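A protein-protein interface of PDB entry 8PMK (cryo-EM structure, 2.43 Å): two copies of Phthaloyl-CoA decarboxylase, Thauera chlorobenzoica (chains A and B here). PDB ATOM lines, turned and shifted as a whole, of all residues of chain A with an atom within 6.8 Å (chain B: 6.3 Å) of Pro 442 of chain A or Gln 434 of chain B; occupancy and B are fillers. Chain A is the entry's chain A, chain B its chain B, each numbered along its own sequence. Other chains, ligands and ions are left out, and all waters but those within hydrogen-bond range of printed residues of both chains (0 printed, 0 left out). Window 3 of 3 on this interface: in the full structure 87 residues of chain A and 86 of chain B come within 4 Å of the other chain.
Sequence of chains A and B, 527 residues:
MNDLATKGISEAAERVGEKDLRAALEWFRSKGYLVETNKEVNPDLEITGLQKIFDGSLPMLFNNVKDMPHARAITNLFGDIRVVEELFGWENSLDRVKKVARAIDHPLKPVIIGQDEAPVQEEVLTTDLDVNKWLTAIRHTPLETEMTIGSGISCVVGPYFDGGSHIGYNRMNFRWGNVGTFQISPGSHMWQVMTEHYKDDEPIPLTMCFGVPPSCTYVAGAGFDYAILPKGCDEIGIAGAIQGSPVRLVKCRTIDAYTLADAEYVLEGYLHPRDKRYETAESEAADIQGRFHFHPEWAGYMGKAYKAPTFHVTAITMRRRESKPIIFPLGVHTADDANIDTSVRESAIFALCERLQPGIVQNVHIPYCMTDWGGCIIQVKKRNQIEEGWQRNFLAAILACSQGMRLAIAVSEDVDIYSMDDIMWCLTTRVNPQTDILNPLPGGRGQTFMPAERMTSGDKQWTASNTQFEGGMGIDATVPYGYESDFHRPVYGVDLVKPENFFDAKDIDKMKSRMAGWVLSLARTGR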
ATOM      1  N   ASN A 439       9.911  13.086  30.780  1.00  0.00           N
ATOM      2  CA  ASN A 439       9.959  12.301  29.549  1.00  0.00           C
ATOM      3  C   ASN A 439       8.684  12.624  28.788  1.00  0.00           C
ATOM      4  O   ASN A 439       7.688  11.896  28.894  1.00  0.00           O
ATOM      5  CB  ASN A 439      10.094  10.809  29.836  1.00  0.00           C
ATOM      6  CG  ASN A 439      10.553  10.031  28.631  1.00  0.00           C
ATOM      7  OD1 ASN A 439       9.953   9.025  28.264  1.00  0.00           O
ATOM      8  ND2 ASN A 439      11.617  10.497  27.998  1.00  0.00           N
ATOM      9  N   PRO A 440       8.670  13.729  28.019  1.00  0.00           N
ATOM     10  CA  PRO A 440       7.397  14.276  27.533  1.00  0.00           C
ATOM     11  C   PRO A 440       6.783  13.549  26.350  1.00  0.00           C
ATOM     12  O   PRO A 440       5.560  13.407  26.285  1.00  0.00           O
ATOM     13  CB  PRO A 440       7.764  15.716  27.148  1.00  0.00           C
ATOM     14  CG  PRO A 440       9.162  15.927  27.619  1.00  0.00           C
ATOM     15  CD  PRO A 440       9.795  14.593  27.635  1.00  0.00           C
ATOM     16  N   LEU A 441       7.598  13.081  25.413  1.00  0.00           N
ATOM     17  CA  LEU A 441       7.096  12.492  24.171  1.00  0.00           C
ATOM     18  C   LEU A 441       7.727  11.128  23.863  1.00  0.00           C
ATOM     19  O   LEU A 441       8.441  10.967  22.865  1.00  0.00           O
ATOM     20  CB  LEU A 441       7.262  13.511  23.034  1.00  0.00           C
ATOM     21  CG  LEU A 441       8.559  14.279  22.696  1.00  0.00           C
ATOM     22  CD1 LEU A 441       8.702  14.425  21.214  1.00  0.00           C
ATOM     23  CD2 LEU A 441       8.577  15.654  23.337  1.00  0.00           C
ATOM     24  N   PRO A 442       7.401  10.074  24.665  1.00  0.00           N
ATOM     25  CA  PRO A 442       8.045   8.769  24.467  1.00  0.00           C
ATOM     26  C   PRO A 442       7.428   8.018  23.297  1.00  0.00           C
ATOM     27  O   PRO A 442       6.294   7.535  23.369  1.00  0.00           O
ATOM     28  CB  PRO A 442       7.795   8.052  25.802  1.00  0.00           C
ATOM     29  CG  PRO A 442       6.941   8.979  26.625  1.00  0.00           C
ATOM     30  CD  PRO A 442       6.348   9.957  25.687  1.00  0.00           C
ATOM     31  N   GLY A 443       8.181   7.915  22.213  1.00  0.00           N
ATOM     32  CA  GLY A 443       7.676   7.343  20.990  1.00  0.00           C
ATOM     33  C   GLY A 443       7.416   8.333  19.885  1.00  0.00           C
ATOM     34  O   GLY A 443       6.803   7.963  18.880  1.00  0.00           O
ATOM     35  N   GLY A 444       7.865   9.569  20.031  1.00  0.00           N
ATOM     36  CA  GLY A 444       7.687  10.593  19.024  1.00  0.00           C
ATOM     37  C   GLY A 444       8.765  10.570  17.966  1.00  0.00           C
ATOM     38  O   GLY A 444       9.316   9.521  17.622  1.00  0.00           O
ATOM     39  N   SER A 465       1.432   2.833  17.673  1.00  0.00           N
ATOM     40  CA  SER A 465       1.525   4.133  17.021  1.00  0.00           C
ATOM     41  C   SER A 465       2.652   4.974  17.617  1.00  0.00           C
ATOM     42  O   SER A 465       2.431   6.103  18.050  1.00  0.00           O
ATOM     43  CB  SER A 465       0.186   4.878  17.117  1.00  0.00           C
ATOM     44  OG  SER A 465      -0.437   4.697  18.381  1.00  0.00           O
ATOM     45  N   ASN A 466       3.862   4.416  17.625  1.00  0.00           N
ATOM     46  CA  ASN A 466       5.021   5.096  18.186  1.00  0.00           C
ATOM     47  C   ASN A 466       6.281   4.607  17.485  1.00  0.00           C
ATOM     48  O   ASN A 466       6.299   3.538  16.870  1.00  0.00           O
ATOM     49  CB  ASN A 466       5.128   4.871  19.700  1.00  0.00           C
ATOM     50  CG  ASN A 466       5.115   3.405  20.076  1.00  0.00           C
ATOM     51  OD1 ASN A 466       6.155   2.748  20.101  1.00  0.00           O
ATOM     52  ND2 ASN A 466       3.932   2.884  20.380  1.00  0.00           N
ATOM     53  N   THR A 467       7.338   5.408  17.585  1.00  0.00           N
ATOM     54  CA  THR A 467       8.623   5.105  16.974  1.00  0.00           C
ATOM     55  C   THR A 467       9.607   4.594  18.025  1.00  0.00           C
ATOM     56  O   THR A 467       9.246   4.295  19.167  1.00  0.00           O
ATOM     57  CB  THR A 467       9.196   6.328  16.255  1.00  0.00           C
ATOM     58  OG1 THR A 467       9.832   7.192  17.205  1.00  0.00           O
ATOM     59  CG2 THR A 467       8.109   7.084  15.537  1.00  0.00           C
ATOM     60  N   PHE A 469      12.098   6.384  19.179  1.00  0.00           N
ATOM     61  CA  PHE A 469      12.625   7.495  19.961  1.00  0.00           C
ATOM     62  C   PHE A 469      12.170   7.389  21.411  1.00  0.00           C
ATOM     63  O   PHE A 469      10.993   7.143  21.687  1.00  0.00           O
ATOM     64  CB  PHE A 469      12.175   8.826  19.369  1.00  0.00           C
ATOM     65  CG  PHE A 469      12.742  10.021  20.073  1.00  0.00           C
ATOM     66  CD1 PHE A 469      14.113  10.115  20.311  1.00  0.00           C
ATOM     67  CD2 PHE A 469      11.902  11.045  20.508  1.00  0.00           C
ATOM     68  CE1 PHE A 469      14.645  11.223  20.969  1.00  0.00           C
ATOM     69  CE2 PHE A 469      12.419  12.158  21.166  1.00  0.00           C
ATOM     70  CZ  PHE A 469      13.792  12.243  21.395  1.00  0.00           C
ATOM     71  N   GLU A 470      13.108   7.574  22.335  1.00  0.00           N
ATOM     72  CA  GLU A 470      12.840   7.300  23.739  1.00  0.00           C
ATOM     73  C   GLU A 470      12.173   8.457  24.464  1.00  0.00           C
ATOM     74  O   GLU A 470      11.658   8.258  25.568  1.00  0.00           O
ATOM     75  CB  GLU A 470      14.137   6.920  24.444  1.00  0.00           C
ATOM     76  CG  GLU A 470      14.949   5.896  23.684  1.00  0.00           C
ATOM     77  CD  GLU A 470      16.162   6.497  23.014  1.00  0.00           C
ATOM     78  OE1 GLU A 470      16.081   7.664  22.578  1.00  0.00           O
ATOM     79  OE2 GLU A 470      17.198   5.808  22.925  1.00  0.00           O
ATOM     80  N   GLY A 471      12.169   9.654  23.889  1.00  0.00           N
ATOM     81  CA  GLY A 471      11.361  10.712  24.455  1.00  0.00           C
ATOM     82  C   GLY A 471      12.058  12.012  24.780  1.00  0.00           C
ATOM     83  O   GLY A 471      11.407  13.053  24.888  1.00  0.00           O
ATOM     84  N   GLY A 472      13.369  11.976  24.947  1.00  0.00           N
ATOM     85  CA  GLY A 472      14.080  13.132  25.442  1.00  0.00           C
ATOM     86  C   GLY A 472      14.060  13.171  26.954  1.00  0.00           C
ATOM     87  O   GLY A 472      13.434  12.357  27.628  1.00  0.00           O
ATOM     88  N   ASN B 432      19.646   6.081  27.427  1.00  0.00           N
ATOM     89  CA  ASN B 432      18.212   5.887  27.299  1.00  0.00           C
ATOM     90  C   ASN B 432      17.537   6.421  28.556  1.00  0.00           C
ATOM     91  O   ASN B 432      17.870   5.971  29.653  1.00  0.00           O
ATOM     92  CB  ASN B 432      17.900   4.411  27.123  1.00  0.00           C
ATOM     93  CG  ASN B 432      16.603   4.165  26.393  1.00  0.00           C
ATOM     94  OD1 ASN B 432      15.554   4.677  26.772  1.00  0.00           O
ATOM     95  ND2 ASN B 432      16.667   3.365  25.340  1.00  0.00           N
ATOM     96  N   PRO B 433      16.598   7.367  28.452  1.00  0.00           N
ATOM     97  CA  PRO B 433      15.941   7.886  29.665  1.00  0.00           C
ATOM     98  C   PRO B 433      14.933   6.936  30.298  1.00  0.00           C
ATOM     99  O   PRO B 433      14.522   7.179  31.438  1.00  0.00           O
ATOM    100  CB  PRO B 433      15.253   9.162  29.170  1.00  0.00           C
ATOM    101  CG  PRO B 433      15.095   8.964  27.718  1.00  0.00           C
ATOM    102  CD  PRO B 433      16.291   8.197  27.278  1.00  0.00           C
ATOM    103  N   GLN B 434      14.529   5.870  29.612  1.00  0.00           N
ATOM    104  CA  GLN B 434      13.618   4.896  30.190  1.00  0.00           C
ATOM    105  C   GLN B 434      14.344   3.752  30.882  1.00  0.00           C
ATOM    106  O   GLN B 434      13.899   3.288  31.935  1.00  0.00           O
ATOM    107  CB  GLN B 434      12.696   4.342  29.105  1.00  0.00           C
ATOM    108  CG  GLN B 434      11.710   5.357  28.571  1.00  0.00           C
ATOM    109  CD  GLN B 434      11.194   4.988  27.202  1.00  0.00           C
ATOM    110  OE1 GLN B 434      11.673   4.040  26.582  1.00  0.00           O
ATOM    111  NE2 GLN B 434      10.212   5.735  26.720  1.00  0.00           N
ATOM    112  N   THR B 435      15.456   3.280  30.317  1.00  0.00           N
ATOM    113  CA  THR B 435      16.123   2.091  30.830  1.00  0.00           C
ATOM    114  C   THR B 435      17.426   2.360  31.567  1.00  0.00           C
ATOM    115  O   THR B 435      17.764   1.601  32.472  1.00  0.00           O
ATOM    116  CB  THR B 435      16.418   1.103  29.695  1.00  0.00           C
ATOM    117  OG1 THR B 435      17.554   1.552  28.950  1.00  0.00           O
ATOM    118  CG2 THR B 435      15.230   0.970  28.762  1.00  0.00           C
ATOM    119  N   ASP B 436      18.168   3.405  31.212  1.00  0.00           N
ATOM    120  CA  ASP B 436      19.522   3.575  31.725  1.00  0.00           C
ATOM    121  C   ASP B 436      19.602   4.498  32.929  1.00  0.00           C
ATOM    122  O   ASP B 436      20.702   4.917  33.290  1.00  0.00           O
ATOM    123  CB  ASP B 436      20.449   4.093  30.625  1.00  0.00           C
ATOM    124  CG  ASP B 436      20.807   3.028  29.612  1.00  0.00           C
ATOM    125  OD1 ASP B 436      20.210   1.934  29.663  1.00  0.00           O
ATOM    126  OD2 ASP B 436      21.686   3.284  28.763  1.00  0.00           O
ATOM    127  N   ILE B 437      18.481   4.829  33.556  1.00  0.00           N
ATOM    128  CA  ILE B 437      18.479   5.608  34.787  1.00  0.00           C
ATOM    129  C   ILE B 437      18.030   4.694  35.913  1.00  0.00           C
ATOM    130  O   ILE B 437      16.919   4.156  35.878  1.00  0.00           O
ATOM    131  CB  ILE B 437      17.571   6.837  34.689  1.00  0.00           C
ATOM    132  CG1 ILE B 437      18.059   7.763  33.590  1.00  0.00           C
ATOM    133  CG2 ILE B 437      17.550   7.586  36.009  1.00  0.00           C
ATOM    134  CD1 ILE B 437      17.077   8.824  33.279  1.00  0.00           C
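No position is printed for both chains.
Among the printed residues, merely in contact across the chains: Asn 439 of chain A with Pro 433 of chain B (3.8 Å), Asn 439 of chain A with Gln 434 of chain B (3.6 Å), Pro 442 of chain A with Gln 434 of chain B (3.5 Å), Glu 470 of chain A with Pro 433 of chain B (3.8 Å) and Gly 472 of chain A with Pro 433 of chain B (3.8 Å).
Of the 6 printed residues of chain B, 3 touch a printed residue of chain A.
Of the 13 printed residues of chain A, 4 touch a printed residue of chain B.
Hydrophobic or aromatic side chains of chain A within 4 Å of the printed part of chain B: Pro 442.
Among the printed residues, 7 pairs touch across the chains.
The side-chain carboxylate (OE2) of Glu 470 of chain A sits at hydrogen-bond distance from the side-chain amide nitrogen (ND2) of Asn 432 of chain B (3.5 Å).
The backbone carbonyl oxygen (O) of Glu 470 of chain A sits at hydrogen-bond distance from the side-chain amide nitrogen (NE2) of Gln 434 of chain B (3.1 Å).
OD1 of Asn 439 of chain A lies close to O of Glu 470 of chain A, at 3.3 Å.
O of Gly 472 of chain A sits at hydrogen-bond distance from ND2 of Asn 439 of chain A (2.6 Å).
The side-chain amide oxygen (OD1) of Asn 432 of chain B sits close to the backbone NH (N) of Gln 434 of chain B (3.2 Å).
Of the printed residues of chain B, Glu 470 of chain A touches Asn 432 (3.4 Å), Pro 433 (3.8 Å) and Gln 434 (3.1 Å).
Printed residues of chain B within 4 Å of Asn 439 of chain A: Pro 433 (3.8 Å) and Gln 434 (3.6 Å).
Of the printed residues of chain A, Asn 432 of chain B touches Glu 470 (3.4 Å).
Printed residues of chain A within 4 Å of Pro 433 of chain B: Asn 439, Glu 470 and Gly 472.
Of the printed residues of chain B, Gly 472 of chain A touches Pro 433.
Thr 435 of chain B touches none of the printed residues of chain A.
Asn 466 of chain A touches none of the printed residues of chain B.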
